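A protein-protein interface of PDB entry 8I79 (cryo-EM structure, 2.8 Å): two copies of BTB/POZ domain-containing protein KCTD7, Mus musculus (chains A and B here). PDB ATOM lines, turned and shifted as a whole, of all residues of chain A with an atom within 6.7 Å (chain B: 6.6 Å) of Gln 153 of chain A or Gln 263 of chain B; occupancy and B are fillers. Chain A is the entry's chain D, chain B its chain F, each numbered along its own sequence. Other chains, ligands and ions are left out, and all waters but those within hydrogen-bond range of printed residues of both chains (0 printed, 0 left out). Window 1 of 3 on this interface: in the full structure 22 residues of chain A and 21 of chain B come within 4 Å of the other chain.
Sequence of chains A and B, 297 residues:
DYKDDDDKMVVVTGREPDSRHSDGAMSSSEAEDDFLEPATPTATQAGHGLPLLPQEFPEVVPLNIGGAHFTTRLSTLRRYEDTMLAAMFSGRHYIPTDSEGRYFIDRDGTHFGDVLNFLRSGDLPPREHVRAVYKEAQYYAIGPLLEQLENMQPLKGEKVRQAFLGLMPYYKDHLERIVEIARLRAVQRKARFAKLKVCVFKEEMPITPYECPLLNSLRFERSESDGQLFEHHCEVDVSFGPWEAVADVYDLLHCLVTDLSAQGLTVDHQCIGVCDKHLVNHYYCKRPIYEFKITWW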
ATOM      1  N   ARG A 127     -27.229 -17.948  38.938  1.00  0.00           N
ATOM      2  CA  ARG A 127     -26.363 -17.219  38.017  1.00  0.00           C
ATOM      3  C   ARG A 127     -25.088 -16.743  38.702  1.00  0.00           C
ATOM      4  O   ARG A 127     -24.000 -16.811  38.121  1.00  0.00           O
ATOM      5  CB  ARG A 127     -27.126 -16.032  37.434  1.00  0.00           C
ATOM      6  CG  ARG A 127     -26.362 -15.222  36.414  1.00  0.00           C
ATOM      7  CD  ARG A 127     -26.092 -16.057  35.184  1.00  0.00           C
ATOM      8  NE  ARG A 127     -27.346 -16.508  34.596  1.00  0.00           N
ATOM      9  CZ  ARG A 127     -28.085 -15.792  33.762  1.00  0.00           C
ATOM     10  NH1 ARG A 127     -27.742 -14.562  33.418  1.00  0.00           N
ATOM     11  NH2 ARG A 127     -29.206 -16.316  33.275  1.00  0.00           N
ATOM     12  N   VAL A 130     -22.239 -19.525  39.469  1.00  0.00           N
ATOM     13  CA  VAL A 130     -21.748 -20.354  38.370  1.00  0.00           C
ATOM     14  C   VAL A 130     -20.233 -20.496  38.444  1.00  0.00           C
ATOM     15  O   VAL A 130     -19.687 -21.595  38.306  1.00  0.00           O
ATOM     16  CB  VAL A 130     -22.185 -19.766  37.019  1.00  0.00           C
ATOM     17  CG1 VAL A 130     -21.502 -20.497  35.878  1.00  0.00           C
ATOM     18  CG2 VAL A 130     -23.680 -19.831  36.883  1.00  0.00           C
ATOM     19  N   GLN A 148     -22.065 -28.673  32.045  1.00  0.00           N
ATOM     20  CA  GLN A 148     -23.287 -27.890  32.196  1.00  0.00           C
ATOM     21  C   GLN A 148     -22.995 -26.491  32.723  1.00  0.00           C
ATOM     22  O   GLN A 148     -23.782 -25.565  32.499  1.00  0.00           O
ATOM     23  CB  GLN A 148     -24.272 -28.621  33.107  1.00  0.00           C
ATOM     24  CG  GLN A 148     -25.168 -29.605  32.369  1.00  0.00           C
ATOM     25  CD  GLN A 148     -24.611 -31.012  32.349  1.00  0.00           C
ATOM     26  OE1 GLN A 148     -24.500 -31.663  33.386  1.00  0.00           O
ATOM     27  NE2 GLN A 148     -24.245 -31.488  31.164  1.00  0.00           N
ATOM     28  N   LEU A 149     -21.878 -26.314  33.432  1.00  0.00           N
ATOM     29  CA  LEU A 149     -21.509 -24.981  33.896  1.00  0.00           C
ATOM     30  C   LEU A 149     -20.858 -24.161  32.792  1.00  0.00           C
ATOM     31  O   LEU A 149     -21.122 -22.960  32.678  1.00  0.00           O
ATOM     32  CB  LEU A 149     -20.589 -25.089  35.108  1.00  0.00           C
ATOM     33  CG  LEU A 149     -21.302 -25.496  36.396  1.00  0.00           C
ATOM     34  CD1 LEU A 149     -20.312 -25.679  37.520  1.00  0.00           C
ATOM     35  CD2 LEU A 149     -22.349 -24.469  36.776  1.00  0.00           C
ATOM     36  N   GLU A 150     -20.003 -24.781  31.976  1.00  0.00           N
ATOM     37  CA  GLU A 150     -19.469 -24.107  30.800  1.00  0.00           C
ATOM     38  C   GLU A 150     -20.545 -23.800  29.775  1.00  0.00           C
ATOM     39  O   GLU A 150     -20.331 -22.940  28.916  1.00  0.00           O
ATOM     40  CB  GLU A 150     -18.376 -24.957  30.153  1.00  0.00           C
ATOM     41  CG  GLU A 150     -17.064 -24.969  30.909  1.00  0.00           C
ATOM     42  CD  GLU A 150     -16.122 -26.046  30.412  1.00  0.00           C
ATOM     43  OE1 GLU A 150     -16.329 -26.547  29.289  1.00  0.00           O
ATOM     44  OE2 GLU A 150     -15.172 -26.390  31.146  1.00  0.00           O
ATOM     45  N   ASN A 151     -21.683 -24.482  29.839  1.00  0.00           N
ATOM     46  CA  ASN A 151     -22.814 -24.184  28.974  1.00  0.00           C
ATOM     47  C   ASN A 151     -23.708 -23.086  29.532  1.00  0.00           C
ATOM     48  O   ASN A 151     -24.711 -22.744  28.898  1.00  0.00           O
ATOM     49  CB  ASN A 151     -23.642 -25.449  28.737  1.00  0.00           C
ATOM     50  CG  ASN A 151     -24.443 -25.386  27.458  1.00  0.00           C
ATOM     51  OD1 ASN A 151     -24.190 -24.548  26.596  1.00  0.00           O
ATOM     52  ND2 ASN A 151     -25.419 -26.277  27.327  1.00  0.00           N
ATOM     53  N   MET A 152     -23.381 -22.531  30.694  1.00  0.00           N
ATOM     54  CA  MET A 152     -24.187 -21.492  31.315  1.00  0.00           C
ATOM     55  C   MET A 152     -23.517 -20.136  31.115  1.00  0.00           C
ATOM     56  O   MET A 152     -22.319 -20.041  30.847  1.00  0.00           O
ATOM     57  CB  MET A 152     -24.403 -21.802  32.799  1.00  0.00           C
ATOM     58  CG  MET A 152     -25.510 -22.828  33.023  1.00  0.00           C
ATOM     59  SD  MET A 152     -26.111 -22.997  34.712  1.00  0.00           S
ATOM     60  CE  MET A 152     -26.305 -21.284  35.169  1.00  0.00           C
ATOM     61  N   GLN A 153     -24.313 -19.074  31.260  1.00  0.00           N
ATOM     62  CA  GLN A 153     -23.964 -17.794  30.642  1.00  0.00           C
ATOM     63  C   GLN A 153     -22.639 -17.198  31.095  1.00  0.00           C
ATOM     64  O   GLN A 153     -21.847 -16.799  30.223  1.00  0.00           O
ATOM     65  CB  GLN A 153     -25.096 -16.786  30.850  1.00  0.00           C
ATOM     66  CG  GLN A 153     -24.751 -15.378  30.372  1.00  0.00           C
ATOM     67  CD  GLN A 153     -24.143 -15.344  28.978  1.00  0.00           C
ATOM     68  OE1 GLN A 153     -24.463 -16.168  28.124  1.00  0.00           O
ATOM     69  NE2 GLN A 153     -23.251 -14.390  28.749  1.00  0.00           N
ATOM     70  N   PRO A 154     -22.329 -17.078  32.394  1.00  0.00           N
ATOM     71  CA  PRO A 154     -21.076 -16.391  32.758  1.00  0.00           C
ATOM     72  C   PRO A 154     -19.848 -17.014  32.125  1.00  0.00           C
ATOM     73  O   PRO A 154     -18.871 -16.308  31.853  1.00  0.00           O
ATOM     74  CB  PRO A 154     -21.053 -16.500  34.288  1.00  0.00           C
ATOM     75  CG  PRO A 154     -22.477 -16.602  34.666  1.00  0.00           C
ATOM     76  CD  PRO A 154     -23.106 -17.442  33.593  1.00  0.00           C
ATOM     77  N   LEU A 155     -19.879 -18.320  31.862  1.00  0.00           N
ATOM     78  CA  LEU A 155     -18.726 -18.974  31.255  1.00  0.00           C
ATOM     79  C   LEU A 155     -18.893 -19.121  29.748  1.00  0.00           C
ATOM     80  O   LEU A 155     -17.903 -19.233  29.021  1.00  0.00           O
ATOM     81  CB  LEU A 155     -18.496 -20.331  31.915  1.00  0.00           C
ATOM     82  CG  LEU A 155     -18.504 -20.293  33.442  1.00  0.00           C
ATOM     83  CD1 LEU A 155     -18.369 -21.687  34.010  1.00  0.00           C
ATOM     84  CD2 LEU A 155     -17.386 -19.404  33.947  1.00  0.00           C
ATOM     85  N   LYS A 156     -20.133 -19.111  29.255  1.00  0.00           N
ATOM     86  CA  LYS A 156     -20.348 -19.280  27.820  1.00  0.00           C
ATOM     87  C   LYS A 156     -19.821 -18.082  27.034  1.00  0.00           C
ATOM     88  O   LYS A 156     -19.110 -18.246  26.033  1.00  0.00           O
ATOM     89  CB  LYS A 156     -21.833 -19.501  27.542  1.00  0.00           C
ATOM     90  CG  LYS A 156     -22.128 -20.138  26.202  1.00  0.00           C
ATOM     91  CD  LYS A 156     -23.527 -19.791  25.732  1.00  0.00           C
ATOM     92  CE  LYS A 156     -24.583 -20.307  26.686  1.00  0.00           C
ATOM     93  NZ  LYS A 156     -24.972 -21.699  26.344  1.00  0.00           N
ATOM     94  N   GLY A 157     -20.149 -16.869  27.479  1.00  0.00           N
ATOM     95  CA  GLY A 157     -19.610 -15.686  26.829  1.00  0.00           C
ATOM     96  C   GLY A 157     -18.101 -15.600  26.945  1.00  0.00           C
ATOM     97  O   GLY A 157     -17.422 -15.136  26.025  1.00  0.00           O
ATOM     98  N   GLU A 158     -17.554 -16.046  28.077  1.00  0.00           N
ATOM     99  CA  GLU A 158     -16.105 -16.046  28.237  1.00  0.00           C
ATOM    100  C   GLU A 158     -15.440 -17.027  27.282  1.00  0.00           C
ATOM    101  O   GLU A 158     -14.373 -16.737  26.736  1.00  0.00           O
ATOM    102  CB  GLU A 158     -15.728 -16.353  29.685  1.00  0.00           C
ATOM    103  CG  GLU A 158     -15.844 -15.150  30.605  1.00  0.00           C
ATOM    104  CD  GLU A 158     -15.958 -15.536  32.064  1.00  0.00           C
ATOM    105  OE1 GLU A 158     -15.559 -16.666  32.414  1.00  0.00           O
ATOM    106  OE2 GLU A 158     -16.447 -14.710  32.863  1.00  0.00           O
ATOM    107  N   LEU B 175     -35.690 -22.085  21.124  1.00  0.00           N
ATOM    108  CA  LEU B 175     -34.794 -21.213  21.882  1.00  0.00           C
ATOM    109  C   LEU B 175     -33.402 -21.817  21.998  1.00  0.00           C
ATOM    110  O   LEU B 175     -32.394 -21.122  21.807  1.00  0.00           O
ATOM    111  CB  LEU B 175     -35.357 -20.936  23.272  1.00  0.00           C
ATOM    112  CG  LEU B 175     -36.414 -19.852  23.409  1.00  0.00           C
ATOM    113  CD1 LEU B 175     -36.817 -19.728  24.860  1.00  0.00           C
ATOM    114  CD2 LEU B 175     -35.859 -18.545  22.905  1.00  0.00           C
ATOM    115  N   GLU B 176     -33.325 -23.109  22.323  1.00  0.00           N
ATOM    116  CA  GLU B 176     -32.023 -23.757  22.419  1.00  0.00           C
ATOM    117  C   GLU B 176     -31.314 -23.760  21.072  1.00  0.00           C
ATOM    118  O   GLU B 176     -30.094 -23.572  21.003  1.00  0.00           O
ATOM    119  CB  GLU B 176     -32.179 -25.176  22.959  1.00  0.00           C
ATOM    120  CG  GLU B 176     -32.614 -25.230  24.413  1.00  0.00           C
ATOM    121  CD  GLU B 176     -32.865 -26.643  24.898  1.00  0.00           C
ATOM    122  OE1 GLU B 176     -32.634 -27.591  24.119  1.00  0.00           O
ATOM    123  OE2 GLU B 176     -33.296 -26.806  26.059  1.00  0.00           O
ATOM    124  N   VAL B 179     -29.850 -20.237  20.544  1.00  0.00           N
ATOM    125  CA  VAL B 179     -28.651 -20.002  21.346  1.00  0.00           C
ATOM    126  C   VAL B 179     -27.467 -20.775  20.777  1.00  0.00           C
ATOM    127  O   VAL B 179     -26.359 -20.240  20.651  1.00  0.00           O
ATOM    128  CB  VAL B 179     -28.904 -20.366  22.819  1.00  0.00           C
ATOM    129  CG1 VAL B 179     -27.664 -20.093  23.642  1.00  0.00           C
ATOM    130  CG2 VAL B 179     -30.072 -19.572  23.359  1.00  0.00           C
ATOM    131  N   THR B 258     -37.227 -11.709  26.214  1.00  0.00           N
ATOM    132  CA  THR B 258     -37.194 -11.842  27.668  1.00  0.00           C
ATOM    133  C   THR B 258     -36.587 -13.173  28.091  1.00  0.00           C
ATOM    134  O   THR B 258     -35.815 -13.231  29.054  1.00  0.00           O
ATOM    135  CB  THR B 258     -38.598 -11.691  28.249  1.00  0.00           C
ATOM    136  OG1 THR B 258     -39.526 -12.444  27.461  1.00  0.00           O
ATOM    137  CG2 THR B 258     -39.014 -10.231  28.251  1.00  0.00           C
ATOM    138  N   ASP B 259     -36.933 -14.256  27.392  1.00  0.00           N
ATOM    139  CA  ASP B 259     -36.382 -15.560  27.744  1.00  0.00           C
ATOM    140  C   ASP B 259     -34.887 -15.625  27.463  1.00  0.00           C
ATOM    141  O   ASP B 259     -34.128 -16.202  28.250  1.00  0.00           O
ATOM    142  CB  ASP B 259     -37.118 -16.665  26.989  1.00  0.00           C
ATOM    143  CG  ASP B 259     -38.286 -17.224  27.774  1.00  0.00           C
ATOM    144  OD1 ASP B 259     -38.368 -16.957  28.991  1.00  0.00           O
ATOM    145  OD2 ASP B 259     -39.127 -17.927  27.179  1.00  0.00           O
ATOM    146  N   LEU B 260     -34.444 -15.048  26.344  1.00  0.00           N
ATOM    147  CA  LEU B 260     -33.018 -15.034  26.040  1.00  0.00           C
ATOM    148  C   LEU B 260     -32.257 -14.129  26.999  1.00  0.00           C
ATOM    149  O   LEU B 260     -31.151 -14.465  27.434  1.00  0.00           O
ATOM    150  CB  LEU B 260     -32.792 -14.602  24.593  1.00  0.00           C
ATOM    151  CG  LEU B 260     -33.267 -15.580  23.520  1.00  0.00           C
ATOM    152  CD1 LEU B 260     -33.210 -14.944  22.145  1.00  0.00           C
ATOM    153  CD2 LEU B 260     -32.441 -16.844  23.557  1.00  0.00           C
ATOM    154  N   SER B 261     -32.833 -12.975  27.342  1.00  0.00           N
ATOM    155  CA  SER B 261     -32.190 -12.088  28.307  1.00  0.00           C
ATOM    156  C   SER B 261     -32.147 -12.719  29.691  1.00  0.00           C
ATOM    157  O   SER B 261     -31.196 -12.502  30.449  1.00  0.00           O
ATOM    158  CB  SER B 261     -32.912 -10.744  28.353  1.00  0.00           C
ATOM    159  OG  SER B 261     -32.792 -10.060  27.119  1.00  0.00           O
ATOM    160  N   ALA B 262     -33.176 -13.492  30.046  1.00  0.00           N
ATOM    161  CA  ALA B 262     -33.153 -14.216  31.313  1.00  0.00           C
ATOM    162  C   ALA B 262     -32.029 -15.242  31.335  1.00  0.00           C
ATOM    163  O   ALA B 262     -31.506 -15.579  32.404  1.00  0.00           O
ATOM    164  CB  ALA B 262     -34.502 -14.889  31.562  1.00  0.00           C
ATOM    165  N   GLN B 263     -31.650 -15.755  30.165  1.00  0.00           N
ATOM    166  CA  GLN B 263     -30.508 -16.654  30.068  1.00  0.00           C
ATOM    167  C   GLN B 263     -29.180 -15.919  30.163  1.00  0.00           C
ATOM    168  O   GLN B 263     -28.137 -16.574  30.237  1.00  0.00           O
ATOM    169  CB  GLN B 263     -30.566 -17.444  28.761  1.00  0.00           C
ATOM    170  CG  GLN B 263     -31.685 -18.464  28.706  1.00  0.00           C
ATOM    171  CD  GLN B 263     -31.565 -19.389  27.516  1.00  0.00           C
ATOM    172  OE1 GLN B 263     -30.768 -19.154  26.611  1.00  0.00           O
ATOM    173  NE2 GLN B 263     -32.362 -20.449  27.508  1.00  0.00           N
ATOM    174  N   GLY B 264     -29.193 -14.587  30.158  1.00  0.00           N
ATOM    175  CA  GLY B 264     -27.989 -13.793  30.255  1.00  0.00           C
ATOM    176  C   GLY B 264     -27.524 -13.175  28.955  1.00  0.00           C
ATOM    177  O   GLY B 264     -26.663 -12.289  28.987  1.00  0.00           O
ATOM    178  N   LEU B 265     -28.065 -13.606  27.821  1.00  0.00           N
ATOM    179  CA  LEU B 265     -27.635 -13.070  26.539  1.00  0.00           C
ATOM    180  C   LEU B 265     -28.130 -11.640  26.357  1.00  0.00           C
ATOM    181  O   LEU B 265     -29.180 -11.250  26.870  1.00  0.00           O
ATOM    182  CB  LEU B 265     -28.148 -13.944  25.395  1.00  0.00           C
ATOM    183  CG  LEU B 265     -28.141 -15.457  25.612  1.00  0.00           C
ATOM    184  CD1 LEU B 265     -28.700 -16.167  24.394  1.00  0.00           C
ATOM    185  CD2 LEU B 265     -26.746 -15.948  25.913  1.00  0.00           C
ATOM    186  N   THR B 266     -27.353 -10.855  25.616  1.00  0.00           N
ATOM    187  CA  THR B 266     -27.732  -9.498  25.242  1.00  0.00           C
ATOM    188  C   THR B 266     -28.296  -9.538  23.829  1.00  0.00           C
ATOM    189  O   THR B 266     -27.541  -9.655  22.860  1.00  0.00           O
ATOM    190  CB  THR B 266     -26.535  -8.551  25.319  1.00  0.00           C
ATOM    191  OG1 THR B 266     -26.028  -8.525  26.658  1.00  0.00           O
ATOM    192  CG2 THR B 266     -26.943  -7.146  24.912  1.00  0.00           C
ATOM    193  N   THR B 295     -25.124 -10.472  21.545  1.00  0.00           N
ATOM    194  CA  THR B 295     -23.788  -9.956  21.824  1.00  0.00           C
ATOM    195  C   THR B 295     -23.176 -10.772  22.956  1.00  0.00           C
ATOM    196  O   THR B 295     -23.619 -10.684  24.105  1.00  0.00           O
ATOM    197  CB  THR B 295     -23.839  -8.473  22.180  1.00  0.00           C
ATOM    198  OG1 THR B 295     -24.370  -7.734  21.074  1.00  0.00           O
ATOM    199  CG2 THR B 295     -22.451  -7.958  22.497  1.00  0.00           C
ATOM    200  N   TRP B 296     -22.158 -11.566  22.625  1.00  0.00           N
ATOM    201  CA  TRP B 296     -21.531 -12.423  23.625  1.00  0.00           C
ATOM    202  C   TRP B 296     -20.603 -11.631  24.535  1.00  0.00           C
ATOM    203  O   TRP B 296     -20.496 -11.925  25.730  1.00  0.00           O
ATOM    204  CB  TRP B 296     -20.776 -13.552  22.934  1.00  0.00           C
ATOM    205  CG  TRP B 296     -21.671 -14.431  22.142  1.00  0.00           C
ATOM    206  CD1 TRP B 296     -21.799 -14.465  20.790  1.00  0.00           C
ATOM    207  CD2 TRP B 296     -22.583 -15.403  22.656  1.00  0.00           C
ATOM    208  NE1 TRP B 296     -22.730 -15.402  20.426  1.00  0.00           N
ATOM    209  CE2 TRP B 296     -23.228 -15.993  21.556  1.00  0.00           C
ATOM    210  CE3 TRP B 296     -22.916 -15.835  23.942  1.00  0.00           C
ATOM    211  CZ2 TRP B 296     -24.184 -16.990  21.700  1.00  0.00           C
ATOM    212  CZ3 TRP B 296     -23.863 -16.821  24.082  1.00  0.00           C
ATOM    213  CH2 TRP B 296     -24.486 -17.390  22.970  1.00  0.00           C
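Gln 153 of chain A touches three residues of chain B.
Of chain A, only Arg 127 (3.1 Å) and Gln 153 (3.1 Å) come within 4 Å of Gln 263 of chain B.
Of the printed residues of chain A, Gly 264 of chain B touches Arg 127 and Gln 153.
Printed residues of chain A within 4 Å of Trp 296 of chain B: Lys 156 (3.4 Å).
Of the printed residues of chain A, Leu 265 of chain B touches Gln 153 (3.2 Å).
Printed residues of chain A within 4 Å of Ala 262 of chain B: Arg 127 (2.6 Å).
Of the printed residues of chain B, Arg 127 of chain A touches Ala 262 (2.6 Å), Gln 263 (3.1 Å) and Gly 264 (3.3 Å).
The nearest printed residue of chain B that does not touch Arg 127 of chain A is Ser 261 of chain B (5.0 Å).
Among the printed residues, merely in contact across the chains: Arg 127 of chain A with Gly 264 of chain B (3.3 Å), Gln 153 of chain A with Gln 263 of chain B (3.1 Å), Gln 153 of chain A with Gly 264 of chain B (3.6 Å), Gln 153 of chain A with Leu 265 of chain B (3.2 Å) and Lys 156 of chain A with Trp 296 of chain B (3.4 Å).
The backbone carbonyl oxygen (O) of Gln 263 of chain B lies close to the guanidinium group (NH2) of Arg 127 of chain A, at 3.2 Å.
The guanidinium group of Arg 127 of chain A lies within hydrogen-bond range of the backbone carbonyl oxygen of Ala 262 of chain B, 2.6 Å away.
The backbone carbonyl oxygen of Asn 151 of chain A lies within hydrogen-bond range of the side-chain amino group of Lys 156 of chain A (2.8 Å).
The backbone carbonyl oxygen of Leu 260 of chain B is in hydrogen-bond range of the backbone NH of Leu 265 of chain B, 3.2 Å away.
No position is printed for both chains.
Of the 7 pairs that touch across the chains among the printed residues, none has its exchanged pair printed and touching as well.
Of the 13 printed residues of chain A, 3 touch a printed residue of chain B.
Of the 14 printed residues of chain B, 5 touch a printed residue of chain A.
Printed residues of chain B that touch a printed residue of chain A: Ala 262, Gln 263, Gly 264, Leu 265 and Trp 296.
Hydrophobic or aromatic side chains of chain B within 4 Å of the printed part of chain A: Leu 265 and Trp 296.
Among the printed residues, no Asp or Glu carboxylate lies within 4 Å of a Lys or Arg side-chain nitrogen of the other chain.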
